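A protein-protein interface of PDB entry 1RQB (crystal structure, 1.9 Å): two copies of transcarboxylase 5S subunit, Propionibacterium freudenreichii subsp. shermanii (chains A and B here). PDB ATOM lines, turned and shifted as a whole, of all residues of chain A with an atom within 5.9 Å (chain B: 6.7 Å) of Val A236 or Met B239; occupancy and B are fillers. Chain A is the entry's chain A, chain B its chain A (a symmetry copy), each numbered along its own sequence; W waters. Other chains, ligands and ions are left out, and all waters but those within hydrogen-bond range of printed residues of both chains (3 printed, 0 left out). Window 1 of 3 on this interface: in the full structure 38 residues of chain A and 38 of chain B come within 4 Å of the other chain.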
ATOM      1  N   PRO A 203     -15.621  17.389 -19.449  1.00  0.00           N
ATOM      2  CA  PRO A 203     -16.801  18.000 -18.834  1.00  0.00           C
ATOM      3  C   PRO A 203     -16.761  18.319 -17.338  1.00  0.00           C
ATOM      4  O   PRO A 203     -17.084  19.436 -16.940  1.00  0.00           O
ATOM      5  CB  PRO A 203     -17.914  17.009 -19.164  1.00  0.00           C
ATOM      6  CG  PRO A 203     -17.487  16.469 -20.487  1.00  0.00           C
ATOM      7  CD  PRO A 203     -16.005  16.223 -20.262  1.00  0.00           C
ATOM      8  N   GLY A 232     -12.840  15.226 -29.435  1.00  0.00           N
ATOM      9  CA  GLY A 232     -14.266  14.949 -29.523  1.00  0.00           C
ATOM     10  C   GLY A 232     -15.087  15.035 -28.243  1.00  0.00           C
ATOM     11  O   GLY A 232     -16.263  14.679 -28.273  1.00  0.00           O
ATOM     12  N   VAL A 233     -14.525  15.527 -27.135  1.00  0.00           N
ATOM     13  CA  VAL A 233     -15.290  15.560 -25.879  1.00  0.00           C
ATOM     14  C   VAL A 233     -15.678  16.983 -25.465  1.00  0.00           C
ATOM     15  O   VAL A 233     -16.503  17.159 -24.571  1.00  0.00           O
ATOM     16  CB  VAL A 233     -14.458  14.989 -24.663  1.00  0.00           C
ATOM     17  CG1 VAL A 233     -13.747  13.678 -25.047  1.00  0.00           C
ATOM     18  CG2 VAL A 233     -13.405  16.013 -24.202  1.00  0.00           C
ATOM     19  N   THR A 234     -15.133  17.998 -26.124  1.00  0.00           N
ATOM     20  CA  THR A 234     -15.310  19.369 -25.620  1.00  0.00           C
ATOM     21  C   THR A 234     -16.668  20.020 -25.889  1.00  0.00           C
ATOM     22  O   THR A 234     -16.971  21.036 -25.264  1.00  0.00           O
ATOM     23  CB  THR A 234     -14.177  20.290 -26.106  1.00  0.00           C
ATOM     24  OG1 THR A 234     -14.206  20.368 -27.531  1.00  0.00           O
ATOM     25  CG2 THR A 234     -12.818  19.749 -25.635  1.00  0.00           C
ATOM     26  N   GLU A 235     -17.508  19.519 -26.788  1.00  0.00           N
ATOM     27  CA  GLU A 235     -18.793  20.227 -26.891  1.00  0.00           C
ATOM     28  C   GLU A 235     -19.590  19.942 -25.617  1.00  0.00           C
ATOM     29  O   GLU A 235     -20.368  20.767 -25.139  1.00  0.00           O
ATOM     30  CB  GLU A 235     -19.590  19.812 -28.128  1.00  0.00           C
ATOM     31  CG  GLU A 235     -20.841  20.673 -28.297  1.00  0.00           C
ATOM     32  CD  GLU A 235     -21.482  20.517 -29.660  1.00  0.00           C
ATOM     33  OE1 GLU A 235     -20.846  20.888 -30.665  1.00  0.00           O
ATOM     34  OE2 GLU A 235     -22.621  20.023 -29.730  1.00  0.00           O
ATOM     35  N   VAL A 236     -19.382  18.765 -25.042  1.00  0.00           N
ATOM     36  CA  VAL A 236     -20.072  18.459 -23.782  1.00  0.00           C
ATOM     37  C   VAL A 236     -19.454  19.327 -22.683  1.00  0.00           C
ATOM     38  O   VAL A 236     -20.142  19.759 -21.761  1.00  0.00           O
ATOM     39  CB  VAL A 236     -19.932  16.982 -23.426  1.00  0.00           C
ATOM     40  CG1 VAL A 236     -20.696  16.687 -22.126  1.00  0.00           C
ATOM     41  CG2 VAL A 236     -20.497  16.134 -24.569  1.00  0.00           C
ATOM     42  N   SER A 237     -18.153  19.598 -22.797  1.00  0.00           N
ATOM     43  CA  SER A 237     -17.462  20.461 -21.827  1.00  0.00           C
ATOM     44  C   SER A 237     -18.043  21.875 -21.911  1.00  0.00           C
ATOM     45  O   SER A 237     -18.211  22.540 -20.891  1.00  0.00           O
ATOM     46  CB  SER A 237     -15.950  20.484 -22.098  1.00  0.00           C
ATOM     47  OG  SER A 237     -15.411  19.169 -21.966  1.00  0.00           O
ATOM     48  N   LEU A 238     -18.334  22.349 -23.123  1.00  0.00           N
ATOM     49  CA  LEU A 238     -18.942  23.679 -23.282  1.00  0.00           C
ATOM     50  C   LEU A 238     -20.288  23.717 -22.553  1.00  0.00           C
ATOM     51  O   LEU A 238     -20.609  24.691 -21.874  1.00  0.00           O
ATOM     52  CB  LEU A 238     -19.173  24.001 -24.760  1.00  0.00           C
ATOM     53  CG  LEU A 238     -18.110  24.836 -25.475  1.00  0.00           C
ATOM     54  CD1 LEU A 238     -16.764  24.201 -25.342  1.00  0.00           C
ATOM     55  CD2 LEU A 238     -18.492  25.004 -26.940  1.00  0.00           C
ATOM     56  N   MET A 239     -21.085  22.663 -22.697  1.00  0.00           N
ATOM     57  CA  MET A 239     -22.395  22.624 -22.027  1.00  0.00           C
ATOM     58  C   MET A 239     -22.191  22.679 -20.511  1.00  0.00           C
ATOM     59  O   MET A 239     -22.891  23.412 -19.814  1.00  0.00           O
ATOM     60  CB  MET A 239     -23.162  21.347 -22.390  1.00  0.00           C
ATOM     61  CG  MET A 239     -24.532  21.233 -21.711  1.00  0.00           C
ATOM     62  SD  MET A 239     -25.843  22.548 -22.389  1.00  0.00           S
ATOM     63  CE  MET A 239     -25.823  23.787 -20.941  1.00  0.00           C
ATOM     64  N   LYS A 240     -21.246  21.897 -19.990  1.00  0.00           N
ATOM     65  CA  LYS A 240     -20.960  21.904 -18.546  1.00  0.00           C
ATOM     66  C   LYS A 240     -20.403  23.261 -18.110  1.00  0.00           C
ATOM     67  O   LYS A 240     -20.670  23.718 -16.999  1.00  0.00           O
ATOM     68  CB  LYS A 240     -19.964  20.783 -18.181  1.00  0.00           C
ATOM     69  CG  LYS A 240     -20.612  19.412 -18.196  1.00  0.00           C
ATOM     70  CD  LYS A 240     -21.712  19.397 -17.160  1.00  0.00           C
ATOM     71  CE  LYS A 240     -22.487  18.102 -17.149  1.00  0.00           C
ATOM     72  NZ  LYS A 240     -23.674  18.249 -16.260  1.00  0.00           N
ATOM     73  N   ALA A 241     -19.628  23.905 -18.980  1.00  0.00           N
ATOM     74  CA  ALA A 241     -19.067  25.218 -18.632  1.00  0.00           C
ATOM     75  C   ALA A 241     -20.206  26.236 -18.540  1.00  0.00           C
ATOM     76  O   ALA A 241     -20.194  27.126 -17.691  1.00  0.00           O
ATOM     77  CB  ALA A 241     -18.036  25.661 -19.683  1.00  0.00           C
ATOM     78  N   TYR B 207     -33.144  14.439 -22.149  1.00  0.00           N
ATOM     79  CA  TYR B 207     -33.303  14.305 -20.693  1.00  0.00           C
ATOM     80  C   TYR B 207     -34.779  14.109 -20.331  1.00  0.00           C
ATOM     81  O   TYR B 207     -35.133  13.170 -19.619  1.00  0.00           O
ATOM     82  CB  TYR B 207     -32.763  15.568 -20.003  1.00  0.00           C
ATOM     83  CG  TYR B 207     -32.904  15.550 -18.495  1.00  0.00           C
ATOM     84  CD1 TYR B 207     -31.869  15.081 -17.680  1.00  0.00           C
ATOM     85  CD2 TYR B 207     -34.080  15.982 -17.885  1.00  0.00           C
ATOM     86  CE1 TYR B 207     -32.011  15.048 -16.287  1.00  0.00           C
ATOM     87  CE2 TYR B 207     -34.229  15.955 -16.493  1.00  0.00           C
ATOM     88  CZ  TYR B 207     -33.196  15.489 -15.704  1.00  0.00           C
ATOM     89  OH  TYR B 207     -33.346  15.459 -14.338  1.00  0.00           O
ATOM     90  N   LEU B 225     -30.124   4.422 -26.324  1.00  0.00           N
ATOM     91  CA  LEU B 225     -30.271   5.611 -27.178  1.00  0.00           C
ATOM     92  C   LEU B 225     -29.360   5.494 -28.401  1.00  0.00           C
ATOM     93  O   LEU B 225     -28.167   5.216 -28.281  1.00  0.00           O
ATOM     94  CB  LEU B 225     -29.935   6.877 -26.376  1.00  0.00           C
ATOM     95  CG  LEU B 225     -29.951   8.206 -27.128  1.00  0.00           C
ATOM     96  CD1 LEU B 225     -31.359   8.488 -27.655  1.00  0.00           C
ATOM     97  CD2 LEU B 225     -29.491   9.322 -26.189  1.00  0.00           C
ATOM     98  N   THR B 234     -25.808  16.003 -30.771  1.00  0.00           N
ATOM     99  CA  THR B 234     -26.210  14.804 -30.019  1.00  0.00           C
ATOM    100  C   THR B 234     -25.187  14.253 -29.025  1.00  0.00           C
ATOM    101  O   THR B 234     -25.561  13.438 -28.182  1.00  0.00           O
ATOM    102  CB  THR B 234     -26.684  13.687 -30.965  1.00  0.00           C
ATOM    103  OG1 THR B 234     -25.605  13.297 -31.816  1.00  0.00           O
ATOM    104  CG2 THR B 234     -27.870  14.177 -31.809  1.00  0.00           C
ATOM    105  N   GLU B 235     -23.912  14.625 -29.068  1.00  0.00           N
ATOM    106  CA  GLU B 235     -23.065  14.048 -28.013  1.00  0.00           C
ATOM    107  C   GLU B 235     -23.469  14.690 -26.685  1.00  0.00           C
ATOM    108  O   GLU B 235     -23.402  14.076 -25.620  1.00  0.00           O
ATOM    109  CB  GLU B 235     -21.575  14.256 -28.281  1.00  0.00           C
ATOM    110  CG  GLU B 235     -20.718  13.512 -27.258  1.00  0.00           C
ATOM    111  CD  GLU B 235     -19.262  13.425 -27.663  1.00  0.00           C
ATOM    112  OE1 GLU B 235     -18.964  12.776 -28.684  1.00  0.00           O
ATOM    113  OE2 GLU B 235     -18.413  14.006 -26.964  1.00  0.00           O
ATOM    114  N   VAL B 236     -23.914  15.937 -26.744  1.00  0.00           N
ATOM    115  CA  VAL B 236     -24.375  16.586 -25.508  1.00  0.00           C
ATOM    116  C   VAL B 236     -25.692  15.926 -25.091  1.00  0.00           C
ATOM    117  O   VAL B 236     -25.976  15.783 -23.904  1.00  0.00           O
ATOM    118  CB  VAL B 236     -24.582  18.083 -25.720  1.00  0.00           C
ATOM    119  CG1 VAL B 236     -25.024  18.736 -24.402  1.00  0.00           C
ATOM    120  CG2 VAL B 236     -23.269  18.708 -26.199  1.00  0.00           C
ATOM    121  N   SER B 237     -26.486  15.504 -26.077  1.00  0.00           N
ATOM    122  CA  SER B 237     -27.753  14.812 -25.796  1.00  0.00           C
ATOM    123  C   SER B 237     -27.455  13.483 -25.099  1.00  0.00           C
ATOM    124  O   SER B 237     -28.177  13.083 -24.187  1.00  0.00           O
ATOM    125  CB  SER B 237     -28.543  14.574 -27.093  1.00  0.00           C
ATOM    126  OG  SER B 237     -28.860  15.823 -27.706  1.00  0.00           O
ATOM    127  N   LEU B 238     -26.406  12.783 -25.531  1.00  0.00           N
ATOM    128  CA  LEU B 238     -26.025  11.520 -24.879  1.00  0.00           C
ATOM    129  C   LEU B 238     -25.694  11.784 -23.408  1.00  0.00           C
ATOM    130  O   LEU B 238     -26.093  11.024 -22.526  1.00  0.00           O
ATOM    131  CB  LEU B 238     -24.800  10.903 -25.557  1.00  0.00           C
ATOM    132  CG  LEU B 238     -25.046   9.825 -26.613  1.00  0.00           C
ATOM    133  CD1 LEU B 238     -25.963  10.332 -27.680  1.00  0.00           C
ATOM    134  CD2 LEU B 238     -23.717   9.375 -27.204  1.00  0.00           C
ATOM    135  N   MET B 239     -24.956  12.855 -23.136  1.00  0.00           N
ATOM    136  CA  MET B 239     -24.596  13.177 -21.746  1.00  0.00           C
ATOM    137  C   MET B 239     -25.870  13.442 -20.939  1.00  0.00           C
ATOM    138  O   MET B 239     -26.009  12.957 -19.817  1.00  0.00           O
ATOM    139  CB  MET B 239     -23.691  14.413 -21.682  1.00  0.00           C
ATOM    140  CG  MET B 239     -23.290  14.816 -20.258  1.00  0.00           C
ATOM    141  SD  MET B 239     -22.059  13.525 -19.407  1.00  0.00           S
ATOM    142  CE  MET B 239     -23.284  12.644 -18.241  1.00  0.00           C
ATOM    143  N   LYS B 240     -26.799  14.218 -21.496  1.00  0.00           N
ATOM    144  CA  LYS B 240     -28.067  14.504 -20.807  1.00  0.00           C
ATOM    145  C   LYS B 240     -28.898  13.228 -20.650  1.00  0.00           C
ATOM    146  O   LYS B 240     -29.602  13.060 -19.654  1.00  0.00           O
ATOM    147  CB  LYS B 240     -28.878  15.570 -21.575  1.00  0.00           C
ATOM    148  CG  LYS B 240     -28.302  16.962 -21.405  1.00  0.00           C
ATOM    149  CD  LYS B 240     -28.355  17.320 -19.938  1.00  0.00           C
ATOM    150  CE  LYS B 240     -27.723  18.658 -19.639  1.00  0.00           C
ATOM    151  NZ  LYS B 240     -27.626  18.835 -18.162  1.00  0.00           N
ATOM    152  N   ALA B 241     -28.820  12.331 -21.630  1.00  0.00           N
ATOM    153  CA  ALA B 241     -29.583  11.077 -21.539  1.00  0.00           C
ATOM    154  C   ALA B 241     -29.011  10.228 -20.402  1.00  0.00           C
ATOM    155  O   ALA B 241     -29.745   9.553 -19.683  1.00  0.00           O
ATOM    156  CB  ALA B 241     -29.517  10.308 -22.869  1.00  0.00           C
ATOM    157  N   ILE B 242     -27.697  10.272 -20.235  1.00  0.00           N
ATOM    158  CA  ILE B 242     -27.048   9.516 -19.155  1.00  0.00           C
ATOM    159  C   ILE B 242     -27.463  10.124 -17.813  1.00  0.00           C
ATOM    160  O   ILE B 242     -27.732   9.407 -16.851  1.00  0.00           O
ATOM    161  CB  ILE B 242     -25.509   9.530 -19.335  1.00  0.00           C
ATOM    162  CG1 ILE B 242     -25.145   8.635 -20.529  1.00  0.00           C
ATOM    163  CG2 ILE B 242     -24.802   9.058 -18.039  1.00  0.00           C
ATOM    164  CD1 ILE B 242     -23.708   8.785 -21.007  1.00  0.00           C
ATOM    165  N   GLU B 243     -27.546  11.446 -17.738  1.00  0.00           N
ATOM    166  CA  GLU B 243     -27.988  12.071 -16.483  1.00  0.00           C
ATOM    167  C   GLU B 243     -29.438  11.674 -16.191  1.00  0.00           C
ATOM    168  O   GLU B 243     -29.833  11.560 -15.032  1.00  0.00           O
ATOM    169  CB  GLU B 243     -27.847  13.605 -16.552  1.00  0.00           C
ATOM    170  CG  GLU B 243     -26.381  14.067 -16.664  1.00  0.00           C
ATOM    171  CD  GLU B 243     -26.209  15.586 -16.822  1.00  0.00           C
ATOM    172  OE1 GLU B 243     -27.122  16.249 -17.368  1.00  0.00           O
ATOM    173  OE2 GLU B 243     -25.143  16.113 -16.411  1.00  0.00           O
ATOM    174  N   ALA B 244     -30.228  11.435 -17.235  1.00  0.00           N
ATOM    175  CA  ALA B 244     -31.639  11.072 -17.043  1.00  0.00           C
ATOM    176  C   ALA B 244     -31.790   9.580 -16.735  1.00  0.00           C
ATOM    177  O   ALA B 244     -32.885   9.122 -16.416  1.00  0.00           O
ATOM    178  CB  ALA B 244     -32.458  11.444 -18.269  1.00  0.00           C
ATOM    179  N   VAL B 249     -25.855   3.503 -24.692  1.00  0.00           N
ATOM    180  CA  VAL B 249     -25.843   4.474 -25.797  1.00  0.00           C
ATOM    181  C   VAL B 249     -25.047   3.874 -26.959  1.00  0.00           C
ATOM    182  O   VAL B 249     -24.108   3.112 -26.731  1.00  0.00           O
ATOM    183  CB  VAL B 249     -25.250   5.857 -25.365  1.00  0.00           C
ATOM    184  CG1 VAL B 249     -26.166   6.506 -24.291  1.00  0.00           C
ATOM    185  CG2 VAL B 249     -23.845   5.693 -24.826  1.00  0.00           C
ATOM    186  N   MET B 271     -15.268  11.180 -21.936  1.00  0.00           N
ATOM    187  CA  MET B 271     -15.948  12.374 -21.413  1.00  0.00           C
ATOM    188  C   MET B 271     -16.587  12.128 -20.042  1.00  0.00           C
ATOM    189  O   MET B 271     -16.920  13.086 -19.349  1.00  0.00           O
ATOM    190  CB  MET B 271     -17.046  12.835 -22.371  1.00  0.00           C
ATOM    191  CG  MET B 271     -18.270  11.930 -22.401  1.00  0.00           C
ATOM    192  SD  MET B 271     -19.692  12.535 -23.641  1.00  0.00           S
ATOM    193  CE  MET B 271     -21.198  11.514 -22.962  1.00  0.00           C
ATOM    194  N   LEU B 272     -16.763  10.876 -19.627  1.00  0.00           N
ATOM    195  CA  LEU B 272     -17.443  10.605 -18.351  1.00  0.00           C
ATOM    196  C   LEU B 272     -16.514  10.652 -17.134  1.00  0.00           C
ATOM    197  O   LEU B 272     -16.993  10.595 -16.002  1.00  0.00           O
ATOM    198  CB  LEU B 272     -18.114   9.224 -18.398  1.00  0.00           C
ATOM    199  CG  LEU B 272     -19.194   9.041 -19.463  1.00  0.00           C
ATOM    200  CD1 LEU B 272     -19.740   7.604 -19.408  1.00  0.00           C
ATOM    201  CD2 LEU B 272     -20.307  10.050 -19.223  1.00  0.00           C
ATOM    202  N   THR B 275     -17.408  12.180 -13.432  1.00  0.00           N
ATOM    203  CA  THR B 275     -18.824  12.560 -13.312  1.00  0.00           C
ATOM    204  C   THR B 275     -19.588  11.569 -12.429  1.00  0.00           C
ATOM    205  O   THR B 275     -20.733  11.825 -12.058  1.00  0.00           O
ATOM    206  CB  THR B 275     -19.550  12.509 -14.683  1.00  0.00           C
ATOM    207  OG1 THR B 275     -19.534  11.157 -15.169  1.00  0.00           O
ATOM    208  CG2 THR B 275     -18.867  13.426 -15.709  1.00  0.00           C
ATOM    209  N   TYR B 277     -20.213   8.617 -13.597  1.00  0.00           N
ATOM    210  CA  TYR B 277     -20.628   7.609 -14.585  1.00  0.00           C
ATOM    211  C   TYR B 277     -19.375   7.045 -15.253  1.00  0.00           C
ATOM    212  O   TYR B 277     -18.344   7.712 -15.340  1.00  0.00           O
ATOM    213  CB  TYR B 277     -21.510   8.230 -15.674  1.00  0.00           C
ATOM    214  CG  TYR B 277     -22.674   8.992 -15.119  1.00  0.00           C
ATOM    215  CD1 TYR B 277     -22.743  10.382 -15.250  1.00  0.00           C
ATOM    216  CD2 TYR B 277     -23.704   8.333 -14.437  1.00  0.00           C
ATOM    217  CE1 TYR B 277     -23.812  11.103 -14.722  1.00  0.00           C
ATOM    218  CE2 TYR B 277     -24.777   9.047 -13.896  1.00  0.00           C
ATOM    219  CZ  TYR B 277     -24.820  10.436 -14.049  1.00  0.00           C
ATOM    220  OH  TYR B 277     -25.873  11.157 -13.544  1.00  0.00           O
HETATM  221  O   HOH W   1     -22.439  17.007 -29.756  1.00  0.00           O
HETATM  222  O   HOH W   2     -17.235  14.312 -31.004  1.00  0.00           O
HETATM  223  O   HOH W   3     -18.203  16.905 -27.789  1.00  0.00           O
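O of Gly A232 lies close to OE2 of Glu B235 (2.6 Å). The side-chain amino group of Lys A240 lies within salt-bridge range of the side-chain carboxylate of Glu B243.
The backbone carbonyl oxygen (O) of Val A233 is in hydrogen-bond range of the side-chain hydroxyl (OG) of Ser A237, at 3.5 Å. NZ of Lys B240 lies within salt-bridge range of OE1 of Glu B243.
Pro A203 touches Met B271. Val A233 touches Glu B235. Glu A235 touches Val B236. Val A236 touches Glu B235 (CG2 to O, 3.7 Å). Met B239 touches Val A236. CG2 of Val A236 touches SD of Met B271, 3.8 Å away. Met A239 touches Val B236 (CG to CG1, 3.7 Å).
Printed residues of chain B within 4 Å of Val A236: Glu B235 (3.7 Å), Met B239 (3.7 Å) and Met B271 (3.8 Å). Of chain A, only Val A236 (3.7 Å) comes within 4 Å of Met B239. Of the printed residues of chain B, Pro A203 touches Met B271. Of the printed residues of chain B, Met A239 touches Val B236. Of the printed residues of chain B, Gly A232 touches Glu B235 (2.6 Å). Printed residues of chain A within 4 Å of Met B271: Pro A203 and Val A236. Of the printed residues of chain B, Val A233 touches Glu B235 (3.7 Å). Ala B241 touches none of the printed residues of chain A. The nearest printed residue of chain B that does not touch Val A236 is Val B236 (4.02 Å). The nearest residue of chain A that does not touch Met B239 is Lys A240 (4.6 Å). The nearest printed residue of chain A that does not touch Glu B235 is Thr A234 (5.2 Å).
Hydrophobic or aromatic side chains of chain B within 4 Å of the printed part of chain A: Val B236, Met B239 and Met B271. Among the printed residues, 9 pairs touch across the chains. Among the printed residues, Asp or Glu carboxylates within 4 Å of a Lys or Arg side-chain nitrogen of the other chain: Lys A240 with Glu B243.
Glu A235 touches Val B236, and with the chains exchanged Val A236 touches Glu B235. Val A236 touches Met B239, and with the chains exchanged Met A239 touches Val B236. 8 positions are printed for both chains. Of the 9 pairs that touch across the chains among the printed residues, 4 have their exchanged pair printed and touching as well.
Water W1 bridges N of Glu B235 (2.9 Å) and OE2 of Glu A235 (3.0 Å). Water W3 lies within hydrogen-bond range of the backbone NH of Glu A235 (2.9 Å), the backbone carbonyl oxygen of Gly A232 (3.0 Å) and the side-chain carboxylate of Glu B235 (3.0 Å). Water W2 lies within hydrogen-bond range of O of Gly A232 and OE1 of Glu B235.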
